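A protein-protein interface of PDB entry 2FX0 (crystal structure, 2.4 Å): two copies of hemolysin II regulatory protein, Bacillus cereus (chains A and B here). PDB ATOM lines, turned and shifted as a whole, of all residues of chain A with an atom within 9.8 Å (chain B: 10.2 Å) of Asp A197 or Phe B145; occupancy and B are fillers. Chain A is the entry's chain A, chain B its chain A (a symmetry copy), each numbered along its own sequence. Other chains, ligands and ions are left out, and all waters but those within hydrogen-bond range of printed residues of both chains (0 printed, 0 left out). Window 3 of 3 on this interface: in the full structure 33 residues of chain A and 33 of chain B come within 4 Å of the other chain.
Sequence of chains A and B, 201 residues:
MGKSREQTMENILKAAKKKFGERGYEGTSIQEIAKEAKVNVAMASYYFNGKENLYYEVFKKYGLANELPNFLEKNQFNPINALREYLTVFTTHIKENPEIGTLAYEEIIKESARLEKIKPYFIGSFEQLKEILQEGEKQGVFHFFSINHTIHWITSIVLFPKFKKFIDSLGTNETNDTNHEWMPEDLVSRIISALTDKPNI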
ATOM      1  N   GLY A 140     -26.930  43.209  20.098  1.00  0.00           N
ATOM      2  CA  GLY A 140     -28.132  42.631  20.736  1.00  0.00           C
ATOM      3  C   GLY A 140     -28.405  41.172  20.391  1.00  0.00           C
ATOM      4  O   GLY A 140     -29.427  40.615  20.798  1.00  0.00           O
ATOM      5  N   VAL A 141     -27.491  40.549  19.644  1.00  0.00           N
ATOM      6  CA  VAL A 141     -27.646  39.152  19.228  1.00  0.00           C
ATOM      7  C   VAL A 141     -27.113  38.124  20.272  1.00  0.00           C
ATOM      8  O   VAL A 141     -27.636  37.015  20.385  1.00  0.00           O
ATOM      9  CB  VAL A 141     -27.063  38.927  17.791  1.00  0.00           C
ATOM     10  CG1 VAL A 141     -25.525  38.901  17.782  1.00  0.00           C
ATOM     11  CG2 VAL A 141     -27.632  37.681  17.166  1.00  0.00           C
ATOM     12  N   PHE A 142     -26.087  38.503  21.033  1.00  0.00           N
ATOM     13  CA  PHE A 142     -25.544  37.648  22.105  1.00  0.00           C
ATOM     14  C   PHE A 142     -26.004  38.137  23.479  1.00  0.00           C
ATOM     15  O   PHE A 142     -26.160  39.346  23.700  1.00  0.00           O
ATOM     16  CB  PHE A 142     -24.022  37.578  22.063  1.00  0.00           C
ATOM     17  CG  PHE A 142     -23.463  36.928  20.818  1.00  0.00           C
ATOM     18  CD1 PHE A 142     -24.194  35.977  20.104  1.00  0.00           C
ATOM     19  CD2 PHE A 142     -22.184  37.256  20.378  1.00  0.00           C
ATOM     20  CE1 PHE A 142     -23.659  35.387  18.954  1.00  0.00           C
ATOM     21  CE2 PHE A 142     -21.639  36.670  19.232  1.00  0.00           C
ATOM     22  CZ  PHE A 142     -22.368  35.736  18.527  1.00  0.00           C
ATOM     23  N   HIS A 143     -26.269  37.196  24.382  1.00  0.00           N
ATOM     24  CA  HIS A 143     -26.728  37.527  25.721  1.00  0.00           C
ATOM     25  C   HIS A 143     -25.944  36.702  26.728  1.00  0.00           C
ATOM     26  O   HIS A 143     -25.858  35.484  26.587  1.00  0.00           O
ATOM     27  CB  HIS A 143     -28.223  37.253  25.853  1.00  0.00           C
ATOM     28  CG  HIS A 143     -29.045  37.909  24.792  1.00  0.00           C
ATOM     29  ND1 HIS A 143     -29.386  39.244  24.836  1.00  0.00           N
ATOM     30  CD2 HIS A 143     -29.578  37.423  23.647  1.00  0.00           C
ATOM     31  CE1 HIS A 143     -30.097  39.550  23.768  1.00  0.00           C
ATOM     32  NE2 HIS A 143     -30.231  38.461  23.032  1.00  0.00           N
ATOM     33  N   PHE A 144     -25.359  37.367  27.722  1.00  0.00           N
ATOM     34  CA  PHE A 144     -24.618  36.673  28.787  1.00  0.00           C
ATOM     35  C   PHE A 144     -24.442  37.537  30.029  1.00  0.00           C
ATOM     36  O   PHE A 144     -24.364  38.769  29.944  1.00  0.00           O
ATOM     37  CB  PHE A 144     -23.255  36.147  28.303  1.00  0.00           C
ATOM     38  CG  PHE A 144     -22.484  37.123  27.440  1.00  0.00           C
ATOM     39  CD1 PHE A 144     -22.446  36.959  26.042  1.00  0.00           C
ATOM     40  CD2 PHE A 144     -21.789  38.195  28.017  1.00  0.00           C
ATOM     41  CE1 PHE A 144     -21.730  37.856  25.238  1.00  0.00           C
ATOM     42  CE2 PHE A 144     -21.075  39.091  27.220  1.00  0.00           C
ATOM     43  CZ  PHE A 144     -21.036  38.917  25.841  1.00  0.00           C
ATOM     44  N   PHE A 145     -24.399  36.872  31.180  1.00  0.00           N
ATOM     45  CA  PHE A 145     -24.186  37.532  32.465  1.00  0.00           C
ATOM     46  C   PHE A 145     -22.775  38.144  32.518  1.00  0.00           C
ATOM     47  O   PHE A 145     -22.609  39.358  32.731  1.00  0.00           O
ATOM     48  CB  PHE A 145     -24.407  36.523  33.615  1.00  0.00           C
ATOM     49  CG  PHE A 145     -24.184  37.098  34.993  1.00  0.00           C
ATOM     50  CD1 PHE A 145     -22.998  36.853  35.680  1.00  0.00           C
ATOM     51  CD2 PHE A 145     -25.164  37.881  35.602  1.00  0.00           C
ATOM     52  CE1 PHE A 145     -22.784  37.385  36.946  1.00  0.00           C
ATOM     53  CE2 PHE A 145     -24.960  38.415  36.875  1.00  0.00           C
ATOM     54  CZ  PHE A 145     -23.766  38.165  37.547  1.00  0.00           C
ATOM     55  N   TRP A 153     -15.634  29.495  29.625  1.00  0.00           N
ATOM     56  CA  TRP A 153     -16.276  28.236  29.182  1.00  0.00           C
ATOM     57  C   TRP A 153     -16.161  27.918  27.704  1.00  0.00           C
ATOM     58  O   TRP A 153     -16.203  26.746  27.327  1.00  0.00           O
ATOM     59  CB  TRP A 153     -17.743  28.049  29.689  1.00  0.00           C
ATOM     60  CG  TRP A 153     -18.868  28.799  28.982  1.00  0.00           C
ATOM     61  CD1 TRP A 153     -19.546  29.889  29.463  1.00  0.00           C
ATOM     62  CD2 TRP A 153     -19.476  28.487  27.702  1.00  0.00           C
ATOM     63  NE1 TRP A 153     -20.515  30.294  28.556  1.00  0.00           N
ATOM     64  CE2 TRP A 153     -20.493  29.458  27.471  1.00  0.00           C
ATOM     65  CE3 TRP A 153     -19.251  27.497  26.725  1.00  0.00           C
ATOM     66  CZ2 TRP A 153     -21.276  29.474  26.301  1.00  0.00           C
ATOM     67  CZ3 TRP A 153     -20.036  27.514  25.556  1.00  0.00           C
ATOM     68  CH2 TRP A 153     -21.037  28.498  25.360  1.00  0.00           C
ATOM     69  N   LEU A 187     -20.319  21.340  17.660  1.00  0.00           N
ATOM     70  CA  LEU A 187     -19.924  22.242  18.752  1.00  0.00           C
ATOM     71  C   LEU A 187     -20.068  23.749  18.460  1.00  0.00           C
ATOM     72  O   LEU A 187     -20.478  24.517  19.338  1.00  0.00           O
ATOM     73  CB  LEU A 187     -18.496  21.918  19.224  1.00  0.00           C
ATOM     74  CG  LEU A 187     -17.868  22.750  20.351  1.00  0.00           C
ATOM     75  CD1 LEU A 187     -18.700  22.698  21.630  1.00  0.00           C
ATOM     76  CD2 LEU A 187     -16.439  22.303  20.620  1.00  0.00           C
ATOM     77  N   SER A 189     -22.244  25.211  16.366  1.00  0.00           N
ATOM     78  CA  SER A 189     -23.675  25.471  16.460  1.00  0.00           C
ATOM     79  C   SER A 189     -24.196  25.439  17.897  1.00  0.00           C
ATOM     80  O   SER A 189     -25.064  26.228  18.259  1.00  0.00           O
ATOM     81  CB  SER A 189     -24.452  24.505  15.571  1.00  0.00           C
ATOM     82  OG  SER A 189     -24.339  24.899  14.217  1.00  0.00           O
ATOM     83  N   ARG A 190     -23.655  24.541  18.713  1.00  0.00           N
ATOM     84  CA  ARG A 190     -23.978  24.488  20.141  1.00  0.00           C
ATOM     85  C   ARG A 190     -23.596  25.779  20.871  1.00  0.00           C
ATOM     86  O   ARG A 190     -24.350  26.258  21.706  1.00  0.00           O
ATOM     87  CB  ARG A 190     -23.282  23.302  20.815  1.00  0.00           C
ATOM     88  CG  ARG A 190     -23.657  21.936  20.277  1.00  0.00           C
ATOM     89  CD  ARG A 190     -22.804  20.863  20.948  1.00  0.00           C
ATOM     90  NE  ARG A 190     -22.795  19.604  20.209  1.00  0.00           N
ATOM     91  CZ  ARG A 190     -21.888  18.644  20.374  1.00  0.00           C
ATOM     92  NH1 ARG A 190     -21.963  17.531  19.658  1.00  0.00           N
ATOM     93  NH2 ARG A 190     -20.902  18.793  21.250  1.00  0.00           N
ATOM     94  N   ILE A 191     -22.420  26.327  20.568  1.00  0.00           N
ATOM     95  CA  ILE A 191     -21.958  27.553  21.221  1.00  0.00           C
ATOM     96  C   ILE A 191     -22.803  28.755  20.802  1.00  0.00           C
ATOM     97  O   ILE A 191     -23.275  29.515  21.651  1.00  0.00           O
ATOM     98  CB  ILE A 191     -20.443  27.808  20.992  1.00  0.00           C
ATOM     99  CG1 ILE A 191     -19.620  26.734  21.715  1.00  0.00           C
ATOM    100  CG2 ILE A 191     -20.046  29.186  21.508  1.00  0.00           C
ATOM    101  CD1 ILE A 191     -18.144  26.730  21.374  1.00  0.00           C
ATOM    102  N   ILE A 192     -23.005  28.909  19.494  1.00  0.00           N
ATOM    103  CA  ILE A 192     -23.895  29.954  18.956  1.00  0.00           C
ATOM    104  C   ILE A 192     -25.268  29.895  19.629  1.00  0.00           C
ATOM    105  O   ILE A 192     -25.800  30.920  20.040  1.00  0.00           O
ATOM    106  CB  ILE A 192     -24.082  29.829  17.421  1.00  0.00           C
ATOM    107  CG1 ILE A 192     -22.731  29.814  16.691  1.00  0.00           C
ATOM    108  CG2 ILE A 192     -25.006  30.930  16.880  1.00  0.00           C
ATOM    109  CD1 ILE A 192     -21.948  31.109  16.757  1.00  0.00           C
ATOM    110  N   SER A 193     -25.831  28.698  19.758  1.00  0.00           N
ATOM    111  CA  SER A 193     -27.169  28.572  20.317  1.00  0.00           C
ATOM    112  C   SER A 193     -27.231  28.977  21.786  1.00  0.00           C
ATOM    113  O   SER A 193     -28.215  29.574  22.235  1.00  0.00           O
ATOM    114  CB  SER A 193     -27.723  27.154  20.139  1.00  0.00           C
ATOM    115  OG  SER A 193     -28.963  27.031  20.822  1.00  0.00           O
ATOM    116  N   ALA A 194     -26.194  28.626  22.533  1.00  0.00           N
ATOM    117  CA  ALA A 194     -26.097  28.989  23.951  1.00  0.00           C
ATOM    118  C   ALA A 194     -26.066  30.512  24.080  1.00  0.00           C
ATOM    119  O   ALA A 194     -26.788  31.095  24.902  1.00  0.00           O
ATOM    120  CB  ALA A 194     -24.857  28.370  24.573  1.00  0.00           C
ATOM    121  N   LEU A 195     -25.259  31.143  23.232  1.00  0.00           N
ATOM    122  CA  LEU A 195     -25.058  32.583  23.294  1.00  0.00           C
ATOM    123  C   LEU A 195     -26.290  33.391  22.931  1.00  0.00           C
ATOM    124  O   LEU A 195     -26.607  34.377  23.594  1.00  0.00           O
ATOM    125  CB  LEU A 195     -23.883  32.986  22.414  1.00  0.00           C
ATOM    126  CG  LEU A 195     -22.510  32.582  22.960  1.00  0.00           C
ATOM    127  CD1 LEU A 195     -21.475  32.942  21.937  1.00  0.00           C
ATOM    128  CD2 LEU A 195     -22.200  33.254  24.294  1.00  0.00           C
ATOM    129  N   THR A 196     -26.992  32.952  21.893  1.00  0.00           N
ATOM    130  CA  THR A 196     -28.122  33.689  21.341  1.00  0.00           C
ATOM    131  C   THR A 196     -29.409  33.544  22.142  1.00  0.00           C
ATOM    132  O   THR A 196     -30.343  34.342  21.967  1.00  0.00           O
ATOM    133  CB  THR A 196     -28.399  33.275  19.893  1.00  0.00           C
ATOM    134  OG1 THR A 196     -28.576  31.858  19.832  1.00  0.00           O
ATOM    135  CG2 THR A 196     -27.240  33.687  18.988  1.00  0.00           C
ATOM    136  N   ASP A 197     -29.458  32.533  23.007  1.00  0.00           N
ATOM    137  CA  ASP A 197     -30.636  32.248  23.819  1.00  0.00           C
ATOM    138  C   ASP A 197     -30.941  33.364  24.802  1.00  0.00           C
ATOM    139  O   ASP A 197     -30.038  34.021  25.298  1.00  0.00           O
ATOM    140  CB  ASP A 197     -30.448  30.950  24.581  1.00  0.00           C
ATOM    141  CG  ASP A 197     -31.743  30.418  25.143  1.00  0.00           C
ATOM    142  OD1 ASP A 197     -32.492  29.783  24.376  1.00  0.00           O
ATOM    143  OD2 ASP A 197     -32.012  30.627  26.347  1.00  0.00           O
ATOM    144  N   LYS A 198     -32.225  33.567  25.084  1.00  0.00           N
ATOM    145  CA  LYS A 198     -32.666  34.666  25.928  1.00  0.00           C
ATOM    146  C   LYS A 198     -33.585  34.173  27.047  1.00  0.00           C
ATOM    147  O   LYS A 198     -34.516  33.392  26.818  1.00  0.00           O
ATOM    148  CB  LYS A 198     -33.369  35.717  25.073  1.00  0.00           C
ATOM    149  CG  LYS A 198     -33.284  37.138  25.599  1.00  0.00           C
ATOM    150  CD  LYS A 198     -34.049  38.099  24.688  1.00  0.00           C
ATOM    151  CE  LYS A 198     -33.725  39.540  25.031  1.00  0.00           C
ATOM    152  NZ  LYS A 198     -34.221  40.497  24.005  1.00  0.00           N
ATOM    153  N   GLN B 134     -28.026  21.098  40.535  1.00  0.00           N
ATOM    154  CA  GLN B 134     -29.322  20.575  40.102  1.00  0.00           C
ATOM    155  C   GLN B 134     -30.422  20.662  41.175  1.00  0.00           C
ATOM    156  O   GLN B 134     -31.580  20.902  40.836  1.00  0.00           O
ATOM    157  CB  GLN B 134     -29.181  19.158  39.576  1.00  0.00           C
ATOM    158  CG  GLN B 134     -28.424  19.067  38.242  1.00  0.00           C
ATOM    159  CD  GLN B 134     -28.259  17.628  37.770  1.00  0.00           C
ATOM    160  OE1 GLN B 134     -27.947  16.730  38.565  1.00  0.00           O
ATOM    161  NE2 GLN B 134     -28.472  17.400  36.472  1.00  0.00           N
ATOM    162  N   GLU B 137     -31.400  24.206  41.028  1.00  0.00           N
ATOM    163  CA  GLU B 137     -32.258  24.442  39.867  1.00  0.00           C
ATOM    164  C   GLU B 137     -33.674  23.925  40.121  1.00  0.00           C
ATOM    165  O   GLU B 137     -34.650  24.624  39.875  1.00  0.00           O
ATOM    166  CB  GLU B 137     -31.675  23.787  38.625  1.00  0.00           C
ATOM    167  CG  GLU B 137     -32.393  24.156  37.342  1.00  0.00           C
ATOM    168  CD  GLU B 137     -31.732  23.545  36.100  1.00  0.00           C
ATOM    169  OE1 GLU B 137     -31.054  22.489  36.209  1.00  0.00           O
ATOM    170  OE2 GLU B 137     -31.894  24.128  35.008  1.00  0.00           O
ATOM    171  N   PHE B 142     -31.477  28.456  41.418  1.00  0.00           N
ATOM    172  CA  PHE B 142     -30.408  28.573  40.407  1.00  0.00           C
ATOM    173  C   PHE B 142     -30.990  28.562  38.994  1.00  0.00           C
ATOM    174  O   PHE B 142     -31.992  27.883  38.728  1.00  0.00           O
ATOM    175  CB  PHE B 142     -29.368  27.468  40.548  1.00  0.00           C
ATOM    176  CG  PHE B 142     -28.591  27.507  41.845  1.00  0.00           C
ATOM    177  CD1 PHE B 142     -28.393  28.701  42.538  1.00  0.00           C
ATOM    178  CD2 PHE B 142     -28.035  26.338  42.356  1.00  0.00           C
ATOM    179  CE1 PHE B 142     -27.672  28.717  43.737  1.00  0.00           C
ATOM    180  CE2 PHE B 142     -27.309  26.342  43.551  1.00  0.00           C
ATOM    181  CZ  PHE B 142     -27.123  27.524  44.235  1.00  0.00           C
ATOM    182  N   HIS B 143     -30.394  29.350  38.103  1.00  0.00           N
ATOM    183  CA  HIS B 143     -30.857  29.442  36.728  1.00  0.00           C
ATOM    184  C   HIS B 143     -29.659  29.358  35.799  1.00  0.00           C
ATOM    185  O   HIS B 143     -28.690  30.093  35.980  1.00  0.00           O
ATOM    186  CB  HIS B 143     -31.615  30.749  36.510  1.00  0.00           C
ATOM    187  CG  HIS B 143     -32.714  30.972  37.496  1.00  0.00           C
ATOM    188  ND1 HIS B 143     -33.943  30.357  37.392  1.00  0.00           N
ATOM    189  CD2 HIS B 143     -32.766  31.727  38.619  1.00  0.00           C
ATOM    190  CE1 HIS B 143     -34.706  30.726  38.403  1.00  0.00           C
ATOM    191  NE2 HIS B 143     -34.016  31.560  39.160  1.00  0.00           N
ATOM    192  N   PHE B 144     -29.717  28.452  34.825  1.00  0.00           N
ATOM    193  CA  PHE B 144     -28.642  28.314  33.829  1.00  0.00           C
ATOM    194  C   PHE B 144     -29.103  27.580  32.576  1.00  0.00           C
ATOM    195  O   PHE B 144     -29.988  26.719  32.631  1.00  0.00           O
ATOM    196  CB  PHE B 144     -27.388  27.642  34.415  1.00  0.00           C
ATOM    197  CG  PHE B 144     -27.680  26.445  35.297  1.00  0.00           C
ATOM    198  CD1 PHE B 144     -27.620  26.565  36.698  1.00  0.00           C
ATOM    199  CD2 PHE B 144     -28.001  25.203  34.733  1.00  0.00           C
ATOM    200  CE1 PHE B 144     -27.883  25.461  37.519  1.00  0.00           C
ATOM    201  CE2 PHE B 144     -28.265  24.100  35.548  1.00  0.00           C
ATOM    202  CZ  PHE B 144     -28.196  24.224  36.931  1.00  0.00           C
ATOM    203  N   PHE B 145     -28.497  27.949  31.451  1.00  0.00           N
ATOM    204  CA  PHE B 145     -28.776  27.319  30.163  1.00  0.00           C
ATOM    205  C   PHE B 145     -28.318  25.850  30.182  1.00  0.00           C
ATOM    206  O   PHE B 145     -29.114  24.926  29.945  1.00  0.00           O
ATOM    207  CB  PHE B 145     -28.084  28.112  29.031  1.00  0.00           C
ATOM    208  CG  PHE B 145     -28.286  27.527  27.654  1.00  0.00           C
ATOM    209  CD1 PHE B 145     -27.285  26.770  27.052  1.00  0.00           C
ATOM    210  CD2 PHE B 145     -29.477  27.739  26.960  1.00  0.00           C
ATOM    211  CE1 PHE B 145     -27.467  26.224  25.786  1.00  0.00           C
ATOM    212  CE2 PHE B 145     -29.667  27.199  25.688  1.00  0.00           C
ATOM    213  CZ  PHE B 145     -28.658  26.439  25.102  1.00  0.00           C
ATOM    214  N   SER B 146     -27.043  25.657  30.497  1.00  0.00           N
ATOM    215  CA  SER B 146     -26.415  24.342  30.459  1.00  0.00           C
ATOM    216  C   SER B 146     -25.745  24.019  31.785  1.00  0.00           C
ATOM    217  O   SER B 146     -24.863  24.752  32.247  1.00  0.00           O
ATOM    218  CB  SER B 146     -25.379  24.284  29.333  1.00  0.00           C
ATOM    219  OG  SER B 146     -24.346  23.359  29.635  1.00  0.00           O
ATOM    220  N   ILE B 147     -26.167  22.915  32.397  1.00  0.00           N
ATOM    221  CA  ILE B 147     -25.505  22.442  33.604  1.00  0.00           C
ATOM    222  C   ILE B 147     -24.019  22.187  33.300  1.00  0.00           C
ATOM    223  O   ILE B 147     -23.147  22.573  34.080  1.00  0.00           O
ATOM    224  CB  ILE B 147     -26.246  21.226  34.234  1.00  0.00           C
ATOM    225  CG1 ILE B 147     -25.409  20.578  35.353  1.00  0.00           C
ATOM    226  CG2 ILE B 147     -26.632  20.194  33.173  1.00  0.00           C
ATOM    227  CD1 ILE B 147     -25.463  21.300  36.696  1.00  0.00           C
ATOM    228  N   ASN B 148     -23.742  21.611  32.128  1.00  0.00           N
ATOM    229  CA  ASN B 148     -22.374  21.356  31.668  1.00  0.00           C
ATOM    230  C   ASN B 148     -21.439  22.571  31.625  1.00  0.00           C
ATOM    231  O   ASN B 148     -20.317  22.508  32.161  1.00  0.00           O
ATOM    232  CB  ASN B 148     -22.391  20.677  30.297  1.00  0.00           C
ATOM    233  CG  ASN B 148     -23.034  19.310  30.338  1.00  0.00           C
ATOM    234  OD1 ASN B 148     -23.393  18.809  31.403  1.00  0.00           O
ATOM    235  ND2 ASN B 148     -23.184  18.695  29.176  1.00  0.00           N
ATOM    236  N   HIS B 149     -21.875  23.661  30.980  1.00  0.00           N
ATOM    237  CA  HIS B 149     -21.029  24.855  30.863  1.00  0.00           C
ATOM    238  C   HIS B 149     -20.776  25.438  32.238  1.00  0.00           C
ATOM    239  O   HIS B 149     -19.666  25.903  32.523  1.00  0.00           O
ATOM    240  CB  HIS B 149     -21.660  25.933  29.969  1.00  0.00           C
ATOM    241  CG  HIS B 149     -21.957  25.479  28.574  1.00  0.00           C
ATOM    242  ND1 HIS B 149     -21.361  24.372  28.003  1.00  0.00           N
ATOM    243  CD2 HIS B 149     -22.770  26.000  27.627  1.00  0.00           C
ATOM    244  CE1 HIS B 149     -21.812  24.221  26.768  1.00  0.00           C
ATOM    245  NE2 HIS B 149     -22.668  25.195  26.518  1.00  0.00           N
ATOM    246  N   THR B 150     -21.827  25.405  33.077  1.00  0.00           N
ATOM    247  CA  THR B 150     -21.770  25.899  34.452  1.00  0.00           C
ATOM    248  C   THR B 150     -20.758  25.116  35.275  1.00  0.00           C
ATOM    249  O   THR B 150     -20.010  25.690  36.075  1.00  0.00           O
ATOM    250  CB  THR B 150     -23.144  25.818  35.156  1.00  0.00           C
ATOM    251  OG1 THR B 150     -24.125  26.539  34.399  1.00  0.00           O
ATOM    252  CG2 THR B 150     -23.045  26.419  36.529  1.00  0.00           C
ATOM    253  N   ILE B 151     -20.771  23.797  35.093  1.00  0.00           N
ATOM    254  CA  ILE B 151     -19.771  22.941  35.706  1.00  0.00           C
ATOM    255  C   ILE B 151     -18.397  23.303  35.140  1.00  0.00           C
ATOM    256  O   ILE B 151     -17.467  23.595  35.909  1.00  0.00           O
ATOM    257  CB  ILE B 151     -20.095  21.449  35.503  1.00  0.00           C
ATOM    258  CG1 ILE B 151     -21.340  21.084  36.339  1.00  0.00           C
ATOM    259  CG2 ILE B 151     -18.885  20.607  35.883  1.00  0.00           C
ATOM    260  CD1 ILE B 151     -21.898  19.684  36.109  1.00  0.00           C
ATOM    261  N   TRP B 153     -17.310  26.184  33.776  1.00  0.00           N
ATOM    262  CA  TRP B 153     -16.805  27.506  34.213  1.00  0.00           C
ATOM    263  C   TRP B 153     -16.584  27.670  35.704  1.00  0.00           C
ATOM    264  O   TRP B 153     -15.748  28.478  36.112  1.00  0.00           O
ATOM    265  CB  TRP B 153     -17.586  28.723  33.620  1.00  0.00           C
ATOM    266  CG  TRP B 153     -18.931  29.104  34.232  1.00  0.00           C
ATOM    267  CD1 TRP B 153     -20.166  28.891  33.677  1.00  0.00           C
ATOM    268  CD2 TRP B 153     -19.173  29.806  35.478  1.00  0.00           C
ATOM    269  NE1 TRP B 153     -21.160  29.386  34.508  1.00  0.00           N
ATOM    270  CE2 TRP B 153     -20.584  29.947  35.615  1.00  0.00           C
ATOM    271  CE3 TRP B 153     -18.339  30.310  36.497  1.00  0.00           C
ATOM    272  CZ2 TRP B 153     -21.179  30.563  36.733  1.00  0.00           C
ATOM    273  CZ3 TRP B 153     -18.938  30.928  37.613  1.00  0.00           C
ATOM    274  CH2 TRP B 153     -20.346  31.048  37.715  1.00  0.00           C
ATOM    275  N   ALA B 194     -23.979  34.947  40.203  1.00  0.00           N
ATOM    276  CA  ALA B 194     -24.101  34.596  38.784  1.00  0.00           C
ATOM    277  C   ALA B 194     -25.224  33.573  38.612  1.00  0.00           C
ATOM    278  O   ALA B 194     -26.084  33.714  37.729  1.00  0.00           O
ATOM    279  CB  ALA B 194     -22.786  34.043  38.260  1.00  0.00           C
ATOM    280  N   LEU B 195     -25.230  32.575  39.491  1.00  0.00           N
ATOM    281  CA  LEU B 195     -26.185  31.480  39.401  1.00  0.00           C
ATOM    282  C   LEU B 195     -27.621  31.894  39.660  1.00  0.00           C
ATOM    283  O   LEU B 195     -28.531  31.471  38.950  1.00  0.00           O
ATOM    284  CB  LEU B 195     -25.781  30.354  40.341  1.00  0.00           C
ATOM    285  CG  LEU B 195     -24.546  29.563  39.896  1.00  0.00           C
ATOM    286  CD1 LEU B 195     -24.211  28.575  40.972  1.00  0.00           C
ATOM    287  CD2 LEU B 195     -24.768  28.851  38.565  1.00  0.00           C
ATOM    288  N   ASP B 197     -29.030  34.849  39.408  1.00  0.00           N
ATOM    289  CA  ASP B 197     -29.530  35.903  38.531  1.00  0.00           C
ATOM    290  C   ASP B 197     -30.509  35.375  37.499  1.00  0.00           C
ATOM    291  O   ASP B 197     -30.387  34.249  37.042  1.00  0.00           O
ATOM    292  CB  ASP B 197     -28.376  36.587  37.820  1.00  0.00           C
ATOM    293  CG  ASP B 197     -28.781  37.898  37.193  1.00  0.00           C
ATOM    294  OD1 ASP B 197     -28.837  38.902  37.928  1.00  0.00           O
ATOM    295  OD2 ASP B 197     -29.038  37.929  35.969  1.00  0.00           O
ATOM    296  N   LYS B 198     -31.480  36.206  37.129  1.00  0.00           N
ATOM    297  CA  LYS B 198     -32.545  35.797  36.227  1.00  0.00           C
ATOM    298  C   LYS B 198     -32.700  36.782  35.067  1.00  0.00           C
ATOM    299  O   LYS B 198     -32.729  38.003  35.259  1.00  0.00           O
ATOM    300  CB  LYS B 198     -33.853  35.667  37.004  1.00  0.00           C
ATOM    301  CG  LYS B 198     -34.839  34.658  36.444  1.00  0.00           C
ATOM    302  CD  LYS B 198     -36.121  34.636  37.276  1.00  0.00           C
ATOM    303  CE  LYS B 198     -36.979  33.439  36.912  1.00  0.00           C
ATOM    304  NZ  LYS B 198     -38.092  33.219  37.876  1.00  0.00           N
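Hydrophobic or aromatic side chains of chain A that line the printed part of chain B: Phe A145, Trp A153 and Ala A194. Of the 17 printed residues of chain B, 5 touch a printed residue of chain A. Printed residues of chain B that touch a printed residue of chain A: Phe B145, His B149, Trp B153, Ala B194 and Asp B197. Among the printed residues, 6 pairs touch across the chains.
The side-chain hydroxyl of Ser B146 is in hydrogen-bond range of the backbone NH of His B149 (2.8 Å).
Of chain B, only Phe B145 comes within 4 Å of Ala A194. Of chain B, only Phe B145 comes within 4 Å of Asp A197. Phe B145 touches two residues of chain A. No residue of chain A comes within 4 Å of Ser B146. Of the printed residues of chain A, His B149 touches Trp A153 (3.6 Å). Of the printed residues of chain A, Ala B194 touches Phe A145. The nearest residue of chain A that does not touch Phe B145 is Ser A193 (4.3 Å). The nearest printed residue of chain A that does not touch Asp B197 is Phe A144 (7.5 Å).
Phe A145 touches Ala B194. CE2 of Phe A145 touches CG of Asp B197, 3.9 Å away. Trp A153 touches His B149. CB of Trp A153 touches CB of Trp B153 (3.99 Å). CE1 of Phe B145 touches CB of Ala A194 (3.6 Å). Asp A197 touches Phe B145 (CG to CE2, 3.9 Å).
Phe A145 touches Ala B194, and with the chains exchanged Ala A194 touches Phe B145. Phe A145 touches Asp B197, and with the chains exchanged Asp A197 touches Phe B145. Trp A153 touches its own counterpart, Trp B153.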
